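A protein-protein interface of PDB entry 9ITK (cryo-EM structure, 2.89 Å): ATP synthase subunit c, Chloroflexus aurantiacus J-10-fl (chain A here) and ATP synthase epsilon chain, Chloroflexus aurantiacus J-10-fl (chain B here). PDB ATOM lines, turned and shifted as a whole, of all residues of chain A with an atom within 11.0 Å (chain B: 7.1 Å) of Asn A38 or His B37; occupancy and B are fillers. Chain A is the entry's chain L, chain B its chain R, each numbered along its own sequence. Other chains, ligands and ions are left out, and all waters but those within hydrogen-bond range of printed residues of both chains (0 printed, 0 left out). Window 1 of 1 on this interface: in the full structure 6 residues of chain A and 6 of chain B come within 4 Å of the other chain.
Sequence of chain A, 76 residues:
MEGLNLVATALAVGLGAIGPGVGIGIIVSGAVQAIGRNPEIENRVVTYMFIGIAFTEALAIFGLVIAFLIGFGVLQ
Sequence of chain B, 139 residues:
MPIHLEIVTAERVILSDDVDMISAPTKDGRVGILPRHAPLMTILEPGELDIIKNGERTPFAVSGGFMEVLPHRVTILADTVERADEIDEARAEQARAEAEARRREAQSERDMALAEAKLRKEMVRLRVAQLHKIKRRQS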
ATOM      1  N   GLY A  30      31.219 -28.489 -25.211  1.00  0.00           N
ATOM      2  CA  GLY A  30      29.874 -28.451 -25.757  1.00  0.00           C
ATOM      3  C   GLY A  30      28.842 -28.010 -24.739  1.00  0.00           C
ATOM      4  O   GLY A  30      27.917 -27.263 -25.063  1.00  0.00           O
ATOM      5  N   ALA A  31      28.981 -28.470 -23.495  1.00  0.00           N
ATOM      6  CA  ALA A  31      28.048 -28.067 -22.450  1.00  0.00           C
ATOM      7  C   ALA A  31      28.147 -26.575 -22.166  1.00  0.00           C
ATOM      8  O   ALA A  31      27.127 -25.898 -22.009  1.00  0.00           O
ATOM      9  CB  ALA A  31      28.302 -28.872 -21.179  1.00  0.00           C
ATOM     10  N   VAL A  32      29.369 -26.044 -22.110  1.00  0.00           N
ATOM     11  CA  VAL A  32      29.560 -24.636 -21.779  1.00  0.00           C
ATOM     12  C   VAL A  32      28.933 -23.740 -22.841  1.00  0.00           C
ATOM     13  O   VAL A  32      28.347 -22.698 -22.527  1.00  0.00           O
ATOM     14  CB  VAL A  32      31.057 -24.336 -21.588  1.00  0.00           C
ATOM     15  CG1 VAL A  32      31.302 -22.853 -21.623  1.00  0.00           C
ATOM     16  CG2 VAL A  32      31.539 -24.908 -20.276  1.00  0.00           C
ATOM     17  N   GLN A  33      29.040 -24.131 -24.113  1.00  0.00           N
ATOM     18  CA  GLN A  33      28.461 -23.319 -25.179  1.00  0.00           C
ATOM     19  C   GLN A  33      26.952 -23.196 -25.022  1.00  0.00           C
ATOM     20  O   GLN A  33      26.386 -22.117 -25.226  1.00  0.00           O
ATOM     21  CB  GLN A  33      28.810 -23.907 -26.545  1.00  0.00           C
ATOM     22  CG  GLN A  33      30.298 -23.983 -26.822  1.00  0.00           C
ATOM     23  CD  GLN A  33      30.845 -22.724 -27.452  1.00  0.00           C
ATOM     24  OE1 GLN A  33      30.229 -21.662 -27.380  1.00  0.00           O
ATOM     25  NE2 GLN A  33      32.014 -22.833 -28.069  1.00  0.00           N
ATOM     26  N   ALA A  34      26.280 -24.292 -24.663  1.00  0.00           N
ATOM     27  CA  ALA A  34      24.844 -24.222 -24.416  1.00  0.00           C
ATOM     28  C   ALA A  34      24.535 -23.337 -23.218  1.00  0.00           C
ATOM     29  O   ALA A  34      23.543 -22.600 -23.221  1.00  0.00           O
ATOM     30  CB  ALA A  34      24.274 -25.624 -24.210  1.00  0.00           C
ATOM     31  N   ILE A  35      25.369 -23.402 -22.178  1.00  0.00           N
ATOM     32  CA  ILE A  35      25.210 -22.496 -21.043  1.00  0.00           C
ATOM     33  C   ILE A  35      25.353 -21.053 -21.498  1.00  0.00           C
ATOM     34  O   ILE A  35      24.568 -20.181 -21.106  1.00  0.00           O
ATOM     35  CB  ILE A  35      26.223 -22.840 -19.935  1.00  0.00           C
ATOM     36  CG1 ILE A  35      26.107 -24.306 -19.528  1.00  0.00           C
ATOM     37  CG2 ILE A  35      26.008 -21.959 -18.730  1.00  0.00           C
ATOM     38  CD1 ILE A  35      24.698 -24.752 -19.279  1.00  0.00           C
ATOM     39  N   GLY A  36      26.356 -20.774 -22.332  1.00  0.00           N
ATOM     40  CA  GLY A  36      26.521 -19.430 -22.853  1.00  0.00           C
ATOM     41  C   GLY A  36      25.370 -18.992 -23.736  1.00  0.00           C
ATOM     42  O   GLY A  36      24.999 -17.816 -23.740  1.00  0.00           O
ATOM     43  N   ARG A  37      24.790 -19.924 -24.492  1.00  0.00           N
ATOM     44  CA  ARG A  37      23.673 -19.590 -25.368  1.00  0.00           C
ATOM     45  C   ARG A  37      22.389 -19.387 -24.572  1.00  0.00           C
ATOM     46  O   ARG A  37      21.802 -18.301 -24.587  1.00  0.00           O
ATOM     47  CB  ARG A  37      23.492 -20.689 -26.416  1.00  0.00           C
ATOM     48  CG  ARG A  37      22.523 -20.339 -27.524  1.00  0.00           C
ATOM     49  CD  ARG A  37      22.998 -19.131 -28.304  1.00  0.00           C
ATOM     50  NE  ARG A  37      22.118 -18.839 -29.428  1.00  0.00           N
ATOM     51  CZ  ARG A  37      22.348 -19.222 -30.675  1.00  0.00           C
ATOM     52  NH1 ARG A  37      23.428 -19.914 -30.996  1.00  0.00           N
ATOM     53  NH2 ARG A  37      21.475 -18.904 -31.624  1.00  0.00           N
ATOM     54  N   ASN A  38      21.944 -20.424 -23.860  1.00  0.00           N
ATOM     55  CA  ASN A  38      20.714 -20.388 -23.068  1.00  0.00           C
ATOM     56  C   ASN A  38      21.062 -20.667 -21.613  1.00  0.00           C
ATOM     57  O   ASN A  38      21.065 -21.827 -21.176  1.00  0.00           O
ATOM     58  CB  ASN A  38      19.698 -21.403 -23.582  1.00  0.00           C
ATOM     59  CG  ASN A  38      18.708 -20.800 -24.540  1.00  0.00           C
ATOM     60  OD1 ASN A  38      18.285 -19.659 -24.371  1.00  0.00           O
ATOM     61  ND2 ASN A  38      18.315 -21.567 -25.548  1.00  0.00           N
ATOM     62  N   PRO A  39      21.364 -19.634 -20.828  1.00  0.00           N
ATOM     63  CA  PRO A  39      21.685 -19.859 -19.411  1.00  0.00           C
ATOM     64  C   PRO A  39      20.584 -20.548 -18.626  1.00  0.00           C
ATOM     65  O   PRO A  39      20.880 -21.265 -17.664  1.00  0.00           O
ATOM     66  CB  PRO A  39      21.937 -18.439 -18.895  1.00  0.00           C
ATOM     67  CG  PRO A  39      22.464 -17.721 -20.082  1.00  0.00           C
ATOM     68  CD  PRO A  39      21.709 -18.271 -21.260  1.00  0.00           C
ATOM     69  N   GLU A  40      19.322 -20.357 -19.004  1.00  0.00           N
ATOM     70  CA  GLU A  40      18.214 -20.875 -18.212  1.00  0.00           C
ATOM     71  C   GLU A  40      17.935 -22.353 -18.450  1.00  0.00           C
ATOM     72  O   GLU A  40      17.082 -22.918 -17.757  1.00  0.00           O
ATOM     73  CB  GLU A  40      16.947 -20.063 -18.486  1.00  0.00           C
ATOM     74  CG  GLU A  40      17.013 -18.630 -17.985  1.00  0.00           C
ATOM     75  CD  GLU A  40      17.378 -18.539 -16.517  1.00  0.00           C
ATOM     76  OE1 GLU A  40      16.459 -18.577 -15.673  1.00  0.00           O
ATOM     77  OE2 GLU A  40      18.581 -18.428 -16.204  1.00  0.00           O
ATOM     78  N   ILE A  41      18.614 -22.992 -19.396  1.00  0.00           N
ATOM     79  CA  ILE A  41      18.471 -24.425 -19.605  1.00  0.00           C
ATOM     80  C   ILE A  41      19.660 -25.182 -19.001  1.00  0.00           C
ATOM     81  O   ILE A  41      19.942 -26.317 -19.379  1.00  0.00           O
ATOM     82  CB  ILE A  41      18.269 -24.753 -21.095  1.00  0.00           C
ATOM     83  CG1 ILE A  41      17.843 -26.208 -21.310  1.00  0.00           C
ATOM     84  CG2 ILE A  41      19.540 -24.491 -21.873  1.00  0.00           C
ATOM     85  CD1 ILE A  41      17.330 -26.486 -22.694  1.00  0.00           C
ATOM     86  N   GLU A  42      20.356 -24.562 -18.046  1.00  0.00           N
ATOM     87  CA  GLU A  42      21.550 -25.173 -17.472  1.00  0.00           C
ATOM     88  C   GLU A  42      21.229 -26.501 -16.798  1.00  0.00           C
ATOM     89  O   GLU A  42      21.943 -27.491 -16.985  1.00  0.00           O
ATOM     90  CB  GLU A  42      22.198 -24.209 -16.480  1.00  0.00           C
ATOM     91  CG  GLU A  42      23.266 -24.837 -15.609  1.00  0.00           C
ATOM     92  CD  GLU A  42      24.004 -23.814 -14.775  1.00  0.00           C
ATOM     93  OE1 GLU A  42      23.706 -22.610 -14.915  1.00  0.00           O
ATOM     94  OE2 GLU A  42      24.882 -24.210 -13.982  1.00  0.00           O
ATOM     95  N   ASN A  43      20.141 -26.549 -16.029  1.00  0.00           N
ATOM     96  CA  ASN A  43      19.850 -27.742 -15.241  1.00  0.00           C
ATOM     97  C   ASN A  43      19.546 -28.959 -16.104  1.00  0.00           C
ATOM     98  O   ASN A  43      19.551 -30.082 -15.589  1.00  0.00           O
ATOM     99  CB  ASN A  43      18.682 -27.475 -14.288  1.00  0.00           C
ATOM    100  CG  ASN A  43      17.431 -27.016 -15.010  1.00  0.00           C
ATOM    101  OD1 ASN A  43      17.421 -26.869 -16.232  1.00  0.00           O
ATOM    102  ND2 ASN A  43      16.364 -26.791 -14.253  1.00  0.00           N
ATOM    103  N   ARG A  44      19.279 -28.772 -17.396  1.00  0.00           N
ATOM    104  CA  ARG A  44      18.969 -29.903 -18.259  1.00  0.00           C
ATOM    105  C   ARG A  44      20.200 -30.426 -18.992  1.00  0.00           C
ATOM    106  O   ARG A  44      20.436 -31.638 -19.023  1.00  0.00           O
ATOM    107  CB  ARG A  44      17.883 -29.519 -19.266  1.00  0.00           C
ATOM    108  CG  ARG A  44      16.542 -29.221 -18.633  1.00  0.00           C
ATOM    109  CD  ARG A  44      15.436 -29.249 -19.670  1.00  0.00           C
ATOM    110  NE  ARG A  44      15.192 -30.603 -20.149  1.00  0.00           N
ATOM    111  CZ  ARG A  44      14.399 -31.480 -19.547  1.00  0.00           C
ATOM    112  NH1 ARG A  44      13.748 -31.175 -18.435  1.00  0.00           N
ATOM    113  NH2 ARG A  44      14.256 -32.693 -20.072  1.00  0.00           N
ATOM    114  N   VAL A  45      20.987 -29.534 -19.592  1.00  0.00           N
ATOM    115  CA  VAL A  45      22.186 -29.977 -20.296  1.00  0.00           C
ATOM    116  C   VAL A  45      23.229 -30.480 -19.307  1.00  0.00           C
ATOM    117  O   VAL A  45      23.918 -31.474 -19.566  1.00  0.00           O
ATOM    118  CB  VAL A  45      22.739 -28.848 -21.182  1.00  0.00           C
ATOM    119  CG1 VAL A  45      21.846 -28.643 -22.385  1.00  0.00           C
ATOM    120  CG2 VAL A  45      22.862 -27.566 -20.392  1.00  0.00           C
ATOM    121  N   VAL A  46      23.356 -29.813 -18.159  1.00  0.00           N
ATOM    122  CA  VAL A  46      24.346 -30.217 -17.165  1.00  0.00           C
ATOM    123  C   VAL A  46      24.051 -31.621 -16.663  1.00  0.00           C
ATOM    124  O   VAL A  46      24.961 -32.444 -16.503  1.00  0.00           O
ATOM    125  CB  VAL A  46      24.387 -29.200 -16.012  1.00  0.00           C
ATOM    126  CG1 VAL A  46      25.039 -29.811 -14.787  1.00  0.00           C
ATOM    127  CG2 VAL A  46      25.096 -27.937 -16.463  1.00  0.00           C
ATOM    128  N   ILE B   3      10.405 -12.811 -19.758  1.00  0.00           N
ATOM    129  CA  ILE B   3      11.193 -11.902 -20.578  1.00  0.00           C
ATOM    130  C   ILE B   3      10.239 -11.006 -21.356  1.00  0.00           C
ATOM    131  O   ILE B   3       9.192 -11.460 -21.833  1.00  0.00           O
ATOM    132  CB  ILE B   3      12.152 -12.666 -21.518  1.00  0.00           C
ATOM    133  CG1 ILE B   3      13.162 -11.707 -22.150  1.00  0.00           C
ATOM    134  CG2 ILE B   3      11.387 -13.448 -22.580  1.00  0.00           C
ATOM    135  CD1 ILE B   3      14.442 -12.375 -22.591  1.00  0.00           C
ATOM    136  N   VAL B  31      15.193 -21.762 -33.180  1.00  0.00           N
ATOM    137  CA  VAL B  31      15.885 -21.506 -31.924  1.00  0.00           C
ATOM    138  C   VAL B  31      14.859 -21.193 -30.847  1.00  0.00           C
ATOM    139  O   VAL B  31      13.874 -20.489 -31.096  1.00  0.00           O
ATOM    140  CB  VAL B  31      16.908 -20.355 -32.064  1.00  0.00           C
ATOM    141  CG1 VAL B  31      16.220 -19.075 -32.480  1.00  0.00           C
ATOM    142  CG2 VAL B  31      17.667 -20.145 -30.765  1.00  0.00           C
ATOM    143  N   GLY B  32      15.073 -21.742 -29.656  1.00  0.00           N
ATOM    144  CA  GLY B  32      14.266 -21.391 -28.509  1.00  0.00           C
ATOM    145  C   GLY B  32      14.930 -20.305 -27.684  1.00  0.00           C
ATOM    146  O   GLY B  32      16.150 -20.187 -27.646  1.00  0.00           O
ATOM    147  N   ILE B  33      14.106 -19.500 -27.020  1.00  0.00           N
ATOM    148  CA  ILE B  33      14.581 -18.359 -26.250  1.00  0.00           C
ATOM    149  C   ILE B  33      14.036 -18.465 -24.835  1.00  0.00           C
ATOM    150  O   ILE B  33      12.834 -18.673 -24.644  1.00  0.00           O
ATOM    151  CB  ILE B  33      14.159 -17.030 -26.896  1.00  0.00           C
ATOM    152  CG1 ILE B  33      14.799 -16.898 -28.276  1.00  0.00           C
ATOM    153  CG2 ILE B  33      14.564 -15.864 -26.018  1.00  0.00           C
ATOM    154  CD1 ILE B  33      14.249 -15.765 -29.091  1.00  0.00           C
ATOM    155  N   LEU B  34      14.913 -18.321 -23.851  1.00  0.00           N
ATOM    156  CA  LEU B  34      14.566 -18.384 -22.443  1.00  0.00           C
ATOM    157  C   LEU B  34      14.948 -17.083 -21.750  1.00  0.00           C
ATOM    158  O   LEU B  34      15.830 -16.356 -22.222  1.00  0.00           O
ATOM    159  CB  LEU B  34      15.250 -19.576 -21.754  1.00  0.00           C
ATOM    160  CG  LEU B  34      14.628 -20.958 -21.991  1.00  0.00           C
ATOM    161  CD1 LEU B  34      14.859 -21.467 -23.400  1.00  0.00           C
ATOM    162  CD2 LEU B  34      15.145 -21.960 -20.970  1.00  0.00           C
ATOM    163  N   PRO B  35      14.299 -16.760 -20.615  1.00  0.00           N
ATOM    164  CA  PRO B  35      14.396 -15.410 -20.034  1.00  0.00           C
ATOM    165  C   PRO B  35      15.782 -14.785 -19.939  1.00  0.00           C
ATOM    166  O   PRO B  35      15.880 -13.562 -19.811  1.00  0.00           O
ATOM    167  CB  PRO B  35      13.807 -15.601 -18.629  1.00  0.00           C
ATOM    168  CG  PRO B  35      13.016 -16.878 -18.675  1.00  0.00           C
ATOM    169  CD  PRO B  35      13.206 -17.533 -20.006  1.00  0.00           C
ATOM    170  N   ARG B  36      16.850 -15.571 -19.987  1.00  0.00           N
ATOM    171  CA  ARG B  36      18.196 -15.026 -19.856  1.00  0.00           C
ATOM    172  C   ARG B  36      19.048 -15.343 -21.078  1.00  0.00           C
ATOM    173  O   ARG B  36      20.255 -15.561 -20.975  1.00  0.00           O
ATOM    174  CB  ARG B  36      18.864 -15.535 -18.583  1.00  0.00           C
ATOM    175  CG  ARG B  36      18.403 -14.820 -17.323  1.00  0.00           C
ATOM    176  CD  ARG B  36      19.146 -15.317 -16.098  1.00  0.00           C
ATOM    177  NE  ARG B  36      20.578 -15.060 -16.180  1.00  0.00           N
ATOM    178  CZ  ARG B  36      21.495 -15.709 -15.475  1.00  0.00           C
ATOM    179  NH1 ARG B  36      21.165 -16.675 -14.635  1.00  0.00           N
ATOM    180  NH2 ARG B  36      22.776 -15.380 -15.619  1.00  0.00           N
ATOM    181  N   HIS B  37      18.428 -15.336 -22.255  1.00  0.00           N
ATOM    182  CA  HIS B  37      19.128 -15.672 -23.487  1.00  0.00           C
ATOM    183  C   HIS B  37      20.266 -14.693 -23.752  1.00  0.00           C
ATOM    184  O   HIS B  37      20.185 -13.507 -23.426  1.00  0.00           O
ATOM    185  CB  HIS B  37      18.149 -15.667 -24.662  1.00  0.00           C
ATOM    186  CG  HIS B  37      18.622 -16.436 -25.855  1.00  0.00           C
ATOM    187  ND1 HIS B  37      19.769 -16.114 -26.544  1.00  0.00           N
ATOM    188  CD2 HIS B  37      18.088 -17.504 -26.492  1.00  0.00           C
ATOM    189  CE1 HIS B  37      19.929 -16.956 -27.549  1.00  0.00           C
ATOM    190  NE2 HIS B  37      18.922 -17.809 -27.540  1.00  0.00           N
ATOM    191  N   ALA B  38      21.343 -15.209 -24.336  1.00  0.00           N
ATOM    192  CA  ALA B  38      22.488 -14.389 -24.682  1.00  0.00           C
ATOM    193  C   ALA B  38      22.118 -13.405 -25.787  1.00  0.00           C
ATOM    194  O   ALA B  38      21.163 -13.630 -26.531  1.00  0.00           O
ATOM    195  CB  ALA B  38      23.649 -15.269 -25.132  1.00  0.00           C
ATOM    196  N   PRO B  39      22.855 -12.299 -25.905  1.00  0.00           N
ATOM    197  CA  PRO B  39      22.546 -11.321 -26.955  1.00  0.00           C
ATOM    198  C   PRO B  39      22.545 -11.971 -28.327  1.00  0.00           C
ATOM    199  O   PRO B  39      23.387 -12.814 -28.638  1.00  0.00           O
ATOM    200  CB  PRO B  39      23.668 -10.288 -26.822  1.00  0.00           C
ATOM    201  CG  PRO B  39      24.128 -10.401 -25.424  1.00  0.00           C
ATOM    202  CD  PRO B  39      23.898 -11.815 -24.984  1.00  0.00           C
ATOM    203  N   LEU B  40      21.581 -11.572 -29.150  1.00  0.00           N
ATOM    204  CA  LEU B  40      21.338 -12.259 -30.407  1.00  0.00           C
ATOM    205  C   LEU B  40      20.640 -11.306 -31.363  1.00  0.00           C
ATOM    206  O   LEU B  40      19.990 -10.349 -30.937  1.00  0.00           O
ATOM    207  CB  LEU B  40      20.494 -13.516 -30.175  1.00  0.00           C
ATOM    208  CG  LEU B  40      20.251 -14.493 -31.317  1.00  0.00           C
ATOM    209  CD1 LEU B  40      21.380 -15.488 -31.390  1.00  0.00           C
ATOM    210  CD2 LEU B  40      18.939 -15.208 -31.099  1.00  0.00           C
ATOM    211  N   VAL B  69      17.304 -10.229 -29.545  1.00  0.00           N
ATOM    212  CA  VAL B  69      17.127 -10.959 -28.294  1.00  0.00           C
ATOM    213  C   VAL B  69      18.155 -10.416 -27.310  1.00  0.00           C
ATOM    214  O   VAL B  69      19.296 -10.879 -27.250  1.00  0.00           O
ATOM    215  CB  VAL B  69      17.271 -12.469 -28.478  1.00  0.00           C
ATOM    216  CG1 VAL B  69      16.936 -13.186 -27.187  1.00  0.00           C
ATOM    217  CG2 VAL B  69      16.372 -12.939 -29.601  1.00  0.00           C
ATOM    218  N   LEU B  70      17.753  -9.425 -26.533  1.00  0.00           N
ATOM    219  CA  LEU B  70      18.565  -8.935 -25.438  1.00  0.00           C
ATOM    220  C   LEU B  70      18.377  -9.837 -24.222  1.00  0.00           C
ATOM    221  O   LEU B  70      17.414 -10.603 -24.152  1.00  0.00           O
ATOM    222  CB  LEU B  70      18.185  -7.496 -25.111  1.00  0.00           C
ATOM    223  CG  LEU B  70      18.937  -6.421 -25.898  1.00  0.00           C
ATOM    224  CD1 LEU B  70      18.720  -5.052 -25.276  1.00  0.00           C
ATOM    225  CD2 LEU B  70      20.418  -6.745 -25.993  1.00  0.00           C
ATOM    226  N   PRO B  71      19.299  -9.789 -23.256  1.00  0.00           N
ATOM    227  CA  PRO B  71      19.140 -10.641 -22.067  1.00  0.00           C
ATOM    228  C   PRO B  71      17.854 -10.389 -21.301  1.00  0.00           C
ATOM    229  O   PRO B  71      17.330 -11.316 -20.673  1.00  0.00           O
ATOM    230  CB  PRO B  71      20.373 -10.293 -21.223  1.00  0.00           C
ATOM    231  CG  PRO B  71      21.369  -9.804 -22.201  1.00  0.00           C
ATOM    232  CD  PRO B  71      20.590  -9.080 -23.252  1.00  0.00           C
ATOM    233  N   HIS B  72      17.324  -9.166 -21.334  1.00  0.00           N
ATOM    234  CA  HIS B  72      16.143  -8.814 -20.557  1.00  0.00           C
ATOM    235  C   HIS B  72      14.882  -8.634 -21.386  1.00  0.00           C
ATOM    236  O   HIS B  72      13.786  -8.835 -20.861  1.00  0.00           O
ATOM    237  CB  HIS B  72      16.397  -7.526 -19.765  1.00  0.00           C
ATOM    238  CG  HIS B  72      17.182  -6.502 -20.522  1.00  0.00           C
ATOM    239  ND1 HIS B  72      16.629  -5.732 -21.522  1.00  0.00           N
ATOM    240  CD2 HIS B  72      18.479  -6.126 -20.429  1.00  0.00           C
ATOM    241  CE1 HIS B  72      17.551  -4.922 -22.010  1.00  0.00           C
ATOM    242  NE2 HIS B  72      18.682  -5.141 -21.364  1.00  0.00           N
ATOM    243  N   VAL B  74      12.972  -9.106 -25.490  1.00  0.00           N
ATOM    244  CA  VAL B  74      12.992  -9.732 -26.805  1.00  0.00           C
ATOM    245  C   VAL B  74      12.090  -8.926 -27.724  1.00  0.00           C
ATOM    246  O   VAL B  74      10.938  -8.646 -27.377  1.00  0.00           O
ATOM    247  CB  VAL B  74      12.528 -11.198 -26.743  1.00  0.00           C
ATOM    248  CG1 VAL B  74      12.178 -11.700 -28.131  1.00  0.00           C
ATOM    249  CG2 VAL B  74      13.595 -12.063 -26.112  1.00  0.00           C
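Gly A36 touches Ala B38.
Arg A37 touches His B37.
Leu B40 touches Arg A37 (CD1 to NH2, 3.4 Å).
Asn A38 touches Leu B34.
His B37 touches Asn A38.
Pro A39 touches Arg B36 (CD to O, 3.1 Å).
CB of Glu A40 touches CD2 of Leu B34 (3.6 Å).
Ile A41 touches Leu B34.
Asn A38 touches just these residues of chain B: Gly B32, Leu B34 and His B37.
Of chain A, only Arg A37 and Asn A38 come within 4 Å of His B37.
Gly B32 touches one residue of chain A.
Pro B35 touches none of the printed residues of chain A.
Ala B38 touches two residues of chain A.
No residue of chain A comes within 4 Å of Pro B71.
Printed residues of chain B within 4 Å of Glu A40: Leu B34 (3.6 Å) and Arg B36 (3.2 Å).
Of the printed residues of chain B, Arg A37 touches His B37, Ala B38 and Leu B40.
Printed residues of chain A within 4 Å of Arg B36: Pro A39 and Glu A40.
Val B69 touches none of the printed residues of chain A.
Of the 16 printed residues of chain B, 6 touch a printed residue of chain A.
Printed residues of chain B that touch a printed residue of chain A: Gly B32, Leu B34, Arg B36, His B37, Ala B38 and Leu B40.
Hydrophobic or aromatic side chains of chain B within 4 Å of the printed part of chain A: Leu B34, His B37, Ala B38 and Leu B40.
Hydrophobic or aromatic side chains of chain A within 4 Å of the printed part of chain B: Pro A39.
Among the printed residues, 11 pairs touch across the chains.
Among the printed residues, Asp or Glu carboxylates within 4 Å of a Lys or Arg side-chain nitrogen of the other chain: Glu A40 with Arg B36 (3.5 Å).
The backbone carbonyl oxygen (O) of Arg A37 is in hydrogen-bond range of the backbone NH (N) of Ala B38.
ND2 of Asn A38 lies within hydrogen-bond range of O of Gly B32 (3.3 Å).
The guanidinium group (NH1) of Arg B36 lies within salt-bridge range of the side-chain carboxylate (OE2) of Glu A40 (3.5 Å).
The backbone NH (N) of Val B69 is in hydrogen-bond range of the backbone carbonyl oxygen (O) of Leu B40 (3.0 Å).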
